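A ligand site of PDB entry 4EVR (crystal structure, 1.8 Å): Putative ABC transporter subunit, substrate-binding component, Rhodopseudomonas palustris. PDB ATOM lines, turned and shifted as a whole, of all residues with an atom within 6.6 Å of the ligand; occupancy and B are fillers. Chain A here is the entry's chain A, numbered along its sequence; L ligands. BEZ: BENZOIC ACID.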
ATOM      1  N   TYR A  29     -20.403 -22.397 -23.721  1.00  0.00           N
ATOM      2  CA  TYR A  29     -21.693 -23.049 -23.584  1.00  0.00           C
ATOM      3  C   TYR A  29     -21.620 -24.496 -23.097  1.00  0.00           C
ATOM      4  O   TYR A  29     -22.682 -25.152 -23.060  1.00  0.00           O
ATOM      5  CB  TYR A  29     -22.448 -22.990 -24.906  1.00  0.00           C
ATOM      6  CG  TYR A  29     -22.887 -21.587 -25.320  1.00  0.00           C
ATOM      7  CD1 TYR A  29     -23.197 -20.619 -24.354  1.00  0.00           C
ATOM      8  CD2 TYR A  29     -23.160 -21.287 -26.643  1.00  0.00           C
ATOM      9  CE1 TYR A  29     -23.631 -19.360 -24.727  1.00  0.00           C
ATOM     10  CE2 TYR A  29     -23.699 -20.046 -27.018  1.00  0.00           C
ATOM     11  CZ  TYR A  29     -23.989 -19.110 -26.049  1.00  0.00           C
ATOM     12  OH  TYR A  29     -24.522 -17.881 -26.351  1.00  0.00           O
ATOM     13  N   LEU A  32     -24.336 -25.580 -20.733  1.00  0.00           N
ATOM     14  CA  LEU A  32     -25.631 -25.724 -21.387  1.00  0.00           C
ATOM     15  C   LEU A  32     -25.700 -27.107 -21.999  1.00  0.00           C
ATOM     16  O   LEU A  32     -26.687 -27.795 -21.856  1.00  0.00           O
ATOM     17  CB  LEU A  32     -25.880 -24.630 -22.458  1.00  0.00           C
ATOM     18  CG  LEU A  32     -26.270 -23.236 -21.949  1.00  0.00           C
ATOM     19  CD1 LEU A  32     -25.160 -22.580 -20.998  1.00  0.00           C
ATOM     20  CD2 LEU A  32     -26.522 -22.318 -23.093  1.00  0.00           C
ATOM     21  N   THR A  89     -28.919 -28.012 -31.478  1.00  0.00           N
ATOM     22  CA  THR A  89     -27.787 -27.796 -30.578  1.00  0.00           C
ATOM     23  C   THR A  89     -28.079 -26.520 -29.793  1.00  0.00           C
ATOM     24  O   THR A  89     -29.218 -26.067 -29.744  1.00  0.00           O
ATOM     25  CB  THR A  89     -26.471 -27.748 -31.364  1.00  0.00           C
ATOM     26  OG1 THR A  89     -25.420 -27.623 -30.386  1.00  0.00           O
ATOM     27  CG2 THR A  89     -26.445 -26.667 -32.333  1.00  0.00           C
ATOM     28  N   VAL A  90     -27.094 -26.014 -29.132  1.00  0.00           N
ATOM     29  CA  VAL A  90     -27.217 -24.799 -28.305  1.00  0.00           C
ATOM     30  C   VAL A  90     -27.048 -23.508 -29.114  1.00  0.00           C
ATOM     31  O   VAL A  90     -27.881 -22.645 -28.958  1.00  0.00           O
ATOM     32  CB  VAL A  90     -26.235 -24.827 -27.123  1.00  0.00           C
ATOM     33  CG1 VAL A  90     -26.151 -23.498 -26.437  1.00  0.00           C
ATOM     34  CG2 VAL A  90     -26.611 -25.912 -26.171  1.00  0.00           C
ATOM     35  N   HIS A  91     -25.961 -23.362 -29.903  1.00  0.00           N
ATOM     36  CA  HIS A  91     -25.598 -22.132 -30.596  1.00  0.00           C
ATOM     37  C   HIS A  91     -26.394 -22.017 -31.904  1.00  0.00           C
ATOM     38  O   HIS A  91     -26.369 -22.906 -32.728  1.00  0.00           O
ATOM     39  CB  HIS A  91     -24.083 -22.089 -30.849  1.00  0.00           C
ATOM     40  CG  HIS A  91     -23.516 -20.875 -31.493  1.00  0.00           C
ATOM     41  ND1 HIS A  91     -23.791 -20.554 -32.809  1.00  0.00           N
ATOM     42  CD2 HIS A  91     -22.641 -19.968 -31.003  1.00  0.00           C
ATOM     43  CE1 HIS A  91     -23.033 -19.493 -33.083  1.00  0.00           C
ATOM     44  NE2 HIS A  91     -22.277 -19.155 -32.025  1.00  0.00           N
ATOM     45  N   SER A  92     -27.142 -20.925 -32.039  1.00  0.00           N
ATOM     46  CA  SER A  92     -28.009 -20.710 -33.228  1.00  0.00           C
ATOM     47  C   SER A  92     -27.290 -20.753 -34.578  1.00  0.00           C
ATOM     48  O   SER A  92     -27.924 -21.105 -35.569  1.00  0.00           O
ATOM     49  CB  SER A  92     -28.728 -19.369 -33.133  1.00  0.00           C
ATOM     50  OG  SER A  92     -29.899 -19.397 -32.350  1.00  0.00           O
ATOM     51  N   GLY A  93     -26.024 -20.361 -34.649  1.00  0.00           N
ATOM     52  CA  GLY A  93     -25.304 -20.418 -35.938  1.00  0.00           C
ATOM     53  C   GLY A  93     -24.994 -21.853 -36.292  1.00  0.00           C
ATOM     54  O   GLY A  93     -25.295 -22.336 -37.383  1.00  0.00           O
ATOM     55  N   ASN A 113     -32.361 -26.267 -27.738  1.00  0.00           N
ATOM     56  CA  ASN A 113     -32.066 -24.947 -27.236  1.00  0.00           C
ATOM     57  C   ASN A 113     -32.081 -23.907 -28.293  1.00  0.00           C
ATOM     58  O   ASN A 113     -32.844 -22.969 -28.194  1.00  0.00           O
ATOM     59  CB  ASN A 113     -30.734 -24.830 -26.524  1.00  0.00           C
ATOM     60  CG  ASN A 113     -30.564 -23.467 -25.912  1.00  0.00           C
ATOM     61  OD1 ASN A 113     -31.283 -23.093 -24.977  1.00  0.00           O
ATOM     62  ND2 ASN A 113     -29.729 -22.616 -26.497  1.00  0.00           N
ATOM     63  N   ALA A 114     -31.181 -24.004 -29.264  1.00  0.00           N
ATOM     64  CA  ALA A 114     -30.966 -22.937 -30.261  1.00  0.00           C
ATOM     65  C   ALA A 114     -32.258 -22.278 -30.687  1.00  0.00           C
ATOM     66  O   ALA A 114     -33.141 -22.918 -31.235  1.00  0.00           O
ATOM     67  CB  ALA A 114     -30.256 -23.504 -31.459  1.00  0.00           C
ATOM     68  N   GLY A 115     -32.381 -21.003 -30.437  1.00  0.00           N
ATOM     69  CA  GLY A 115     -33.601 -20.245 -30.738  1.00  0.00           C
ATOM     70  C   GLY A 115     -33.648 -19.579 -32.095  1.00  0.00           C
ATOM     71  O   GLY A 115     -34.608 -18.860 -32.355  1.00  0.00           O
ATOM     72  N   ALA A 116     -32.696 -19.882 -32.991  1.00  0.00           N
ATOM     73  CA  ALA A 116     -32.671 -19.263 -34.329  1.00  0.00           C
ATOM     74  C   ALA A 116     -34.096 -19.154 -34.897  1.00  0.00           C
ATOM     75  O   ALA A 116     -34.784 -20.173 -35.035  1.00  0.00           O
ATOM     76  CB  ALA A 116     -31.778 -20.060 -35.268  1.00  0.00           C
ATOM     77  N   PHE A 133     -37.595 -22.510 -27.601  1.00  0.00           N
ATOM     78  CA  PHE A 133     -38.219 -21.207 -27.799  1.00  0.00           C
ATOM     79  C   PHE A 133     -37.688 -20.634 -29.106  1.00  0.00           C
ATOM     80  O   PHE A 133     -36.672 -21.172 -29.622  1.00  0.00           O
ATOM     81  CB  PHE A 133     -37.859 -20.265 -26.654  1.00  0.00           C
ATOM     82  CG  PHE A 133     -36.346 -20.031 -26.581  1.00  0.00           C
ATOM     83  CD1 PHE A 133     -35.512 -20.936 -25.953  1.00  0.00           C
ATOM     84  CD2 PHE A 133     -35.767 -18.937 -27.210  1.00  0.00           C
ATOM     85  CE1 PHE A 133     -34.120 -20.835 -26.113  1.00  0.00           C
ATOM     86  CE2 PHE A 133     -34.406 -18.813 -27.318  1.00  0.00           C
ATOM     87  CZ  PHE A 133     -33.592 -19.776 -26.791  1.00  0.00           C
ATOM     88  N   ASN A 135     -35.934 -17.017 -30.635  1.00  0.00           N
ATOM     89  CA  ASN A 135     -35.194 -15.816 -30.180  1.00  0.00           C
ATOM     90  C   ASN A 135     -36.029 -14.556 -30.198  1.00  0.00           C
ATOM     91  O   ASN A 135     -36.079 -13.802 -29.221  1.00  0.00           O
ATOM     92  CB  ASN A 135     -33.910 -15.595 -31.067  1.00  0.00           C
ATOM     93  CG  ASN A 135     -32.877 -16.580 -30.874  1.00  0.00           C
ATOM     94  OD1 ASN A 135     -32.735 -17.110 -29.751  1.00  0.00           O
ATOM     95  ND2 ASN A 135     -32.036 -16.824 -31.932  1.00  0.00           N
ATOM     96  N   TRP A 159     -23.540 -10.718 -27.726  1.00  0.00           N
ATOM     97  CA  TRP A 159     -22.559 -11.240 -28.693  1.00  0.00           C
ATOM     98  C   TRP A 159     -23.037 -11.027 -30.145  1.00  0.00           C
ATOM     99  O   TRP A 159     -24.274 -11.052 -30.441  1.00  0.00           O
ATOM    100  CB  TRP A 159     -22.325 -12.730 -28.439  1.00  0.00           C
ATOM    101  CG  TRP A 159     -21.427 -13.011 -27.268  1.00  0.00           C
ATOM    102  CD1 TRP A 159     -20.191 -12.500 -27.050  1.00  0.00           C
ATOM    103  CD2 TRP A 159     -21.620 -14.038 -26.274  1.00  0.00           C
ATOM    104  NE1 TRP A 159     -19.587 -13.166 -26.000  1.00  0.00           N
ATOM    105  CE2 TRP A 159     -20.444 -14.103 -25.512  1.00  0.00           C
ATOM    106  CE3 TRP A 159     -22.669 -14.921 -25.968  1.00  0.00           C
ATOM    107  CZ2 TRP A 159     -20.304 -14.975 -24.412  1.00  0.00           C
ATOM    108  CZ3 TRP A 159     -22.520 -15.820 -24.958  1.00  0.00           C
ATOM    109  CH2 TRP A 159     -21.346 -15.842 -24.170  1.00  0.00           C
ATOM    110  N   TYR A 161     -23.718 -12.478 -33.012  1.00  0.00           N
ATOM    111  CA  TYR A 161     -24.103 -13.633 -33.797  1.00  0.00           C
ATOM    112  C   TYR A 161     -25.632 -13.668 -33.838  1.00  0.00           C
ATOM    113  O   TYR A 161     -26.269 -12.898 -33.155  1.00  0.00           O
ATOM    114  CB  TYR A 161     -23.415 -14.932 -33.337  1.00  0.00           C
ATOM    115  CG  TYR A 161     -24.051 -15.627 -32.173  1.00  0.00           C
ATOM    116  CD1 TYR A 161     -24.789 -16.811 -32.348  1.00  0.00           C
ATOM    117  CD2 TYR A 161     -23.774 -15.235 -30.859  1.00  0.00           C
ATOM    118  CE1 TYR A 161     -25.333 -17.499 -31.258  1.00  0.00           C
ATOM    119  CE2 TYR A 161     -24.308 -15.913 -29.765  1.00  0.00           C
ATOM    120  CZ  TYR A 161     -25.035 -17.087 -29.967  1.00  0.00           C
ATOM    121  OH  TYR A 161     -25.647 -17.726 -28.882  1.00  0.00           O
ATOM    122  N   ALA A 162     -26.194 -14.539 -34.629  1.00  0.00           N
ATOM    123  CA  ALA A 162     -27.689 -14.603 -34.849  1.00  0.00           C
ATOM    124  C   ALA A 162     -28.540 -14.571 -33.584  1.00  0.00           C
ATOM    125  O   ALA A 162     -29.529 -13.842 -33.568  1.00  0.00           O
ATOM    126  CB  ALA A 162     -28.047 -15.861 -35.627  1.00  0.00           C
ATOM    127  N   ALA A 163     -28.175 -15.295 -32.514  1.00  0.00           N
ATOM    128  CA  ALA A 163     -28.997 -15.241 -31.304  1.00  0.00           C
ATOM    129  C   ALA A 163     -29.026 -13.874 -30.639  1.00  0.00           C
ATOM    130  O   ALA A 163     -30.108 -13.433 -30.265  1.00  0.00           O
ATOM    131  CB  ALA A 163     -28.570 -16.278 -30.339  1.00  0.00           C
ATOM    132  N   GLY A 164     -27.873 -13.201 -30.490  1.00  0.00           N
ATOM    133  CA  GLY A 164     -27.871 -11.871 -29.920  1.00  0.00           C
ATOM    134  C   GLY A 164     -28.672 -10.924 -30.776  1.00  0.00           C
ATOM    135  O   GLY A 164     -29.528 -10.209 -30.303  1.00  0.00           O
ATOM    136  N   MET A 167     -32.569 -11.789 -30.544  1.00  0.00           N
ATOM    137  CA  MET A 167     -33.138 -11.441 -29.275  1.00  0.00           C
ATOM    138  C   MET A 167     -33.135  -9.911 -29.079  1.00  0.00           C
ATOM    139  O   MET A 167     -34.097  -9.402 -28.488  1.00  0.00           O
ATOM    140  CB  MET A 167     -32.438 -12.156 -28.132  1.00  0.00           C
ATOM    141  CG  MET A 167     -32.914 -13.593 -27.995  1.00  0.00           C
ATOM    142  SD  MET A 167     -32.294 -14.491 -26.477  1.00  0.00           S
ATOM    143  CE  MET A 167     -31.034 -15.735 -27.121  1.00  0.00           C
ATOM    144  N   PHE A 213     -28.023 -10.114 -23.483  1.00  0.00           N
ATOM    145  CA  PHE A 213     -28.069 -11.539 -23.734  1.00  0.00           C
ATOM    146  C   PHE A 213     -26.639 -12.074 -23.681  1.00  0.00           C
ATOM    147  O   PHE A 213     -25.766 -11.769 -24.543  1.00  0.00           O
ATOM    148  CB  PHE A 213     -28.778 -11.926 -25.041  1.00  0.00           C
ATOM    149  CG  PHE A 213     -28.533 -13.398 -25.393  1.00  0.00           C
ATOM    150  CD1 PHE A 213     -28.874 -14.403 -24.503  1.00  0.00           C
ATOM    151  CD2 PHE A 213     -27.710 -13.756 -26.489  1.00  0.00           C
ATOM    152  CE1 PHE A 213     -28.571 -15.744 -24.781  1.00  0.00           C
ATOM    153  CE2 PHE A 213     -27.358 -15.077 -26.702  1.00  0.00           C
ATOM    154  CZ  PHE A 213     -27.719 -16.058 -25.823  1.00  0.00           C
ATOM    155  N   PHE A 214     -26.409 -12.932 -22.691  1.00  0.00           N
ATOM    156  CA  PHE A 214     -25.218 -13.779 -22.574  1.00  0.00           C
ATOM    157  C   PHE A 214     -25.755 -15.081 -21.970  1.00  0.00           C
ATOM    158  O   PHE A 214     -26.858 -15.095 -21.462  1.00  0.00           O
ATOM    159  CB  PHE A 214     -24.078 -13.183 -21.739  1.00  0.00           C
ATOM    160  CG  PHE A 214     -23.478 -11.938 -22.358  1.00  0.00           C
ATOM    161  CD1 PHE A 214     -22.611 -12.030 -23.423  1.00  0.00           C
ATOM    162  CD2 PHE A 214     -23.803 -10.681 -21.881  1.00  0.00           C
ATOM    163  CE1 PHE A 214     -22.087 -10.876 -24.011  1.00  0.00           C
ATOM    164  CE2 PHE A 214     -23.285  -9.550 -22.473  1.00  0.00           C
ATOM    165  CZ  PHE A 214     -22.450  -9.658 -23.548  1.00  0.00           C
ATOM    166  N   SER A 215     -24.973 -16.144 -22.004  1.00  0.00           N
ATOM    167  CA  SER A 215     -25.366 -17.374 -21.368  1.00  0.00           C
ATOM    168  C   SER A 215     -24.082 -18.145 -21.012  1.00  0.00           C
ATOM    169  O   SER A 215     -23.050 -17.865 -21.543  1.00  0.00           O
ATOM    170  CB  SER A 215     -26.266 -18.182 -22.283  1.00  0.00           C
ATOM    171  OG  SER A 215     -26.993 -19.136 -21.545  1.00  0.00           O
ATOM    172  N   GLY A 216     -24.193 -19.102 -20.146  1.00  0.00           N
ATOM    173  CA  GLY A 216     -23.040 -19.940 -19.780  1.00  0.00           C
ATOM    174  C   GLY A 216     -21.942 -19.152 -19.126  1.00  0.00           C
ATOM    175  O   GLY A 216     -22.209 -18.342 -18.242  1.00  0.00           O
ATOM    176  N   PHE A 240     -31.877 -16.742 -19.996  1.00  0.00           N
ATOM    177  CA  PHE A 240     -30.580 -17.406 -20.210  1.00  0.00           C
ATOM    178  C   PHE A 240     -29.470 -16.630 -19.529  1.00  0.00           C
ATOM    179  O   PHE A 240     -28.411 -17.215 -19.230  1.00  0.00           O
ATOM    180  CB  PHE A 240     -30.289 -17.460 -21.715  1.00  0.00           C
ATOM    181  CG  PHE A 240     -31.492 -17.838 -22.520  1.00  0.00           C
ATOM    182  CD1 PHE A 240     -32.078 -19.076 -22.373  1.00  0.00           C
ATOM    183  CD2 PHE A 240     -32.086 -16.935 -23.370  1.00  0.00           C
ATOM    184  CE1 PHE A 240     -33.207 -19.392 -23.042  1.00  0.00           C
ATOM    185  CE2 PHE A 240     -33.213 -17.279 -24.082  1.00  0.00           C
ATOM    186  CZ  PHE A 240     -33.814 -18.469 -23.853  1.00  0.00           C
ATOM    187  N   PHE A 289     -32.342 -25.317 -19.510  1.00  0.00           N
ATOM    188  CA  PHE A 289     -31.607 -26.146 -20.493  1.00  0.00           C
ATOM    189  C   PHE A 289     -31.845 -27.626 -20.189  1.00  0.00           C
ATOM    190  O   PHE A 289     -32.184 -28.422 -21.064  1.00  0.00           O
ATOM    191  CB  PHE A 289     -30.120 -25.801 -20.451  1.00  0.00           C
ATOM    192  CG  PHE A 289     -29.851 -24.306 -20.684  1.00  0.00           C
ATOM    193  CD1 PHE A 289     -30.236 -23.690 -21.857  1.00  0.00           C
ATOM    194  CD2 PHE A 289     -29.386 -23.492 -19.642  1.00  0.00           C
ATOM    195  CE1 PHE A 289     -29.990 -22.352 -22.047  1.00  0.00           C
ATOM    196  CE2 PHE A 289     -29.242 -22.121 -19.818  1.00  0.00           C
ATOM    197  CZ  PHE A 289     -29.549 -21.559 -21.026  1.00  0.00           C
HETATM  198  C   BEZ L   1     -28.645 -19.492 -29.158  1.00  0.00           C
HETATM  199  O1  BEZ L   1     -29.692 -19.744 -29.829  1.00  0.00           O
HETATM  200  O2  BEZ L   1     -27.517 -19.298 -29.690  1.00  0.00           O
HETATM  201  C1  BEZ L   1     -28.673 -19.521 -27.669  1.00  0.00           C
HETATM  202  C2  BEZ L   1     -27.507 -19.822 -26.943  1.00  0.00           C
HETATM  203  C3  BEZ L   1     -27.534 -19.866 -25.557  1.00  0.00           C
HETATM  204  C4  BEZ L   1     -28.742 -19.540 -24.926  1.00  0.00           C
HETATM  205  C5  BEZ L   1     -29.907 -19.246 -25.658  1.00  0.00           C
HETATM  206  C6  BEZ L   1     -29.895 -19.257 -27.028  1.00  0.00           C
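The backbone NH (N) of Ser 92 lies within hydrogen-bond range of an oxygen (O2) of the ligand (2.9 Å). An oxygen (O1) of the ligand lies within hydrogen-bond range of the side-chain hydroxyl of Ser 92 (2.6 Å). An oxygen (O2) of the ligand sits at hydrogen-bond distance from the side-chain hydroxyl (OH) of Tyr 161, at 2.6 Å. An oxygen (O1) of the ligand lies within hydrogen-bond range of the backbone NH (N) of Gly 115 (3.0 Å).
The backbone carbonyl oxygen (O) of Val 90 is in hydrogen-bond range of the side-chain amide nitrogen (ND2) of Asn 113 (3.1 Å). The backbone NH (N) of Ala 116 lies within hydrogen-bond range of the side-chain hydroxyl (OG) of Ser 92. OG of Ser 92 lies within hydrogen-bond range of ND2 of Asn 135 (3.4 Å). OH of Tyr 29 lies within hydrogen-bond range of OH of Tyr 161 (2.8 Å). ND1 of His 91 is in hydrogen-bond range of N of Gly 93 (2.9 Å). O of Phe 240 lies within hydrogen-bond range of OG of Ser 215, at 3.3 Å. N of Ala 114 sits at hydrogen-bond distance from O of Thr 89. O of Gly 115 lies within hydrogen-bond range of N of Asn 135, 2.8 Å away.
An oxygen (O2) of the ligand sits close to the backbone carbonyl oxygen of Val 90 (3.4 Å). Tyr 29 touches the ligand (OH to C2, 3.6 Å). Leu 32 touches the ligand. His 91 touches the ligand (CA to O2, 3.5 Å). Asn 113 touches the ligand (ND2 to C6, 3.4 Å). Ala 114 touches the ligand (CA to O1, 3.5 Å). CZ of Phe 133 touches C6 of the ligand (3.7 Å). Ala 163 touches the ligand. CE of Met 167 touches C6 of the ligand, 3.7 Å away. CZ of Phe 213 touches C4 of the ligand, at 3.7 Å. Ser 215 touches the ligand (OG to C4, 3.8 Å). Phe 240 touches the ligand. Of the 25 residues printed, 15 come within 4 Å of the ligand. The nearest printed residue that does not touch the ligand is Asn 135 (4.03 Å).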
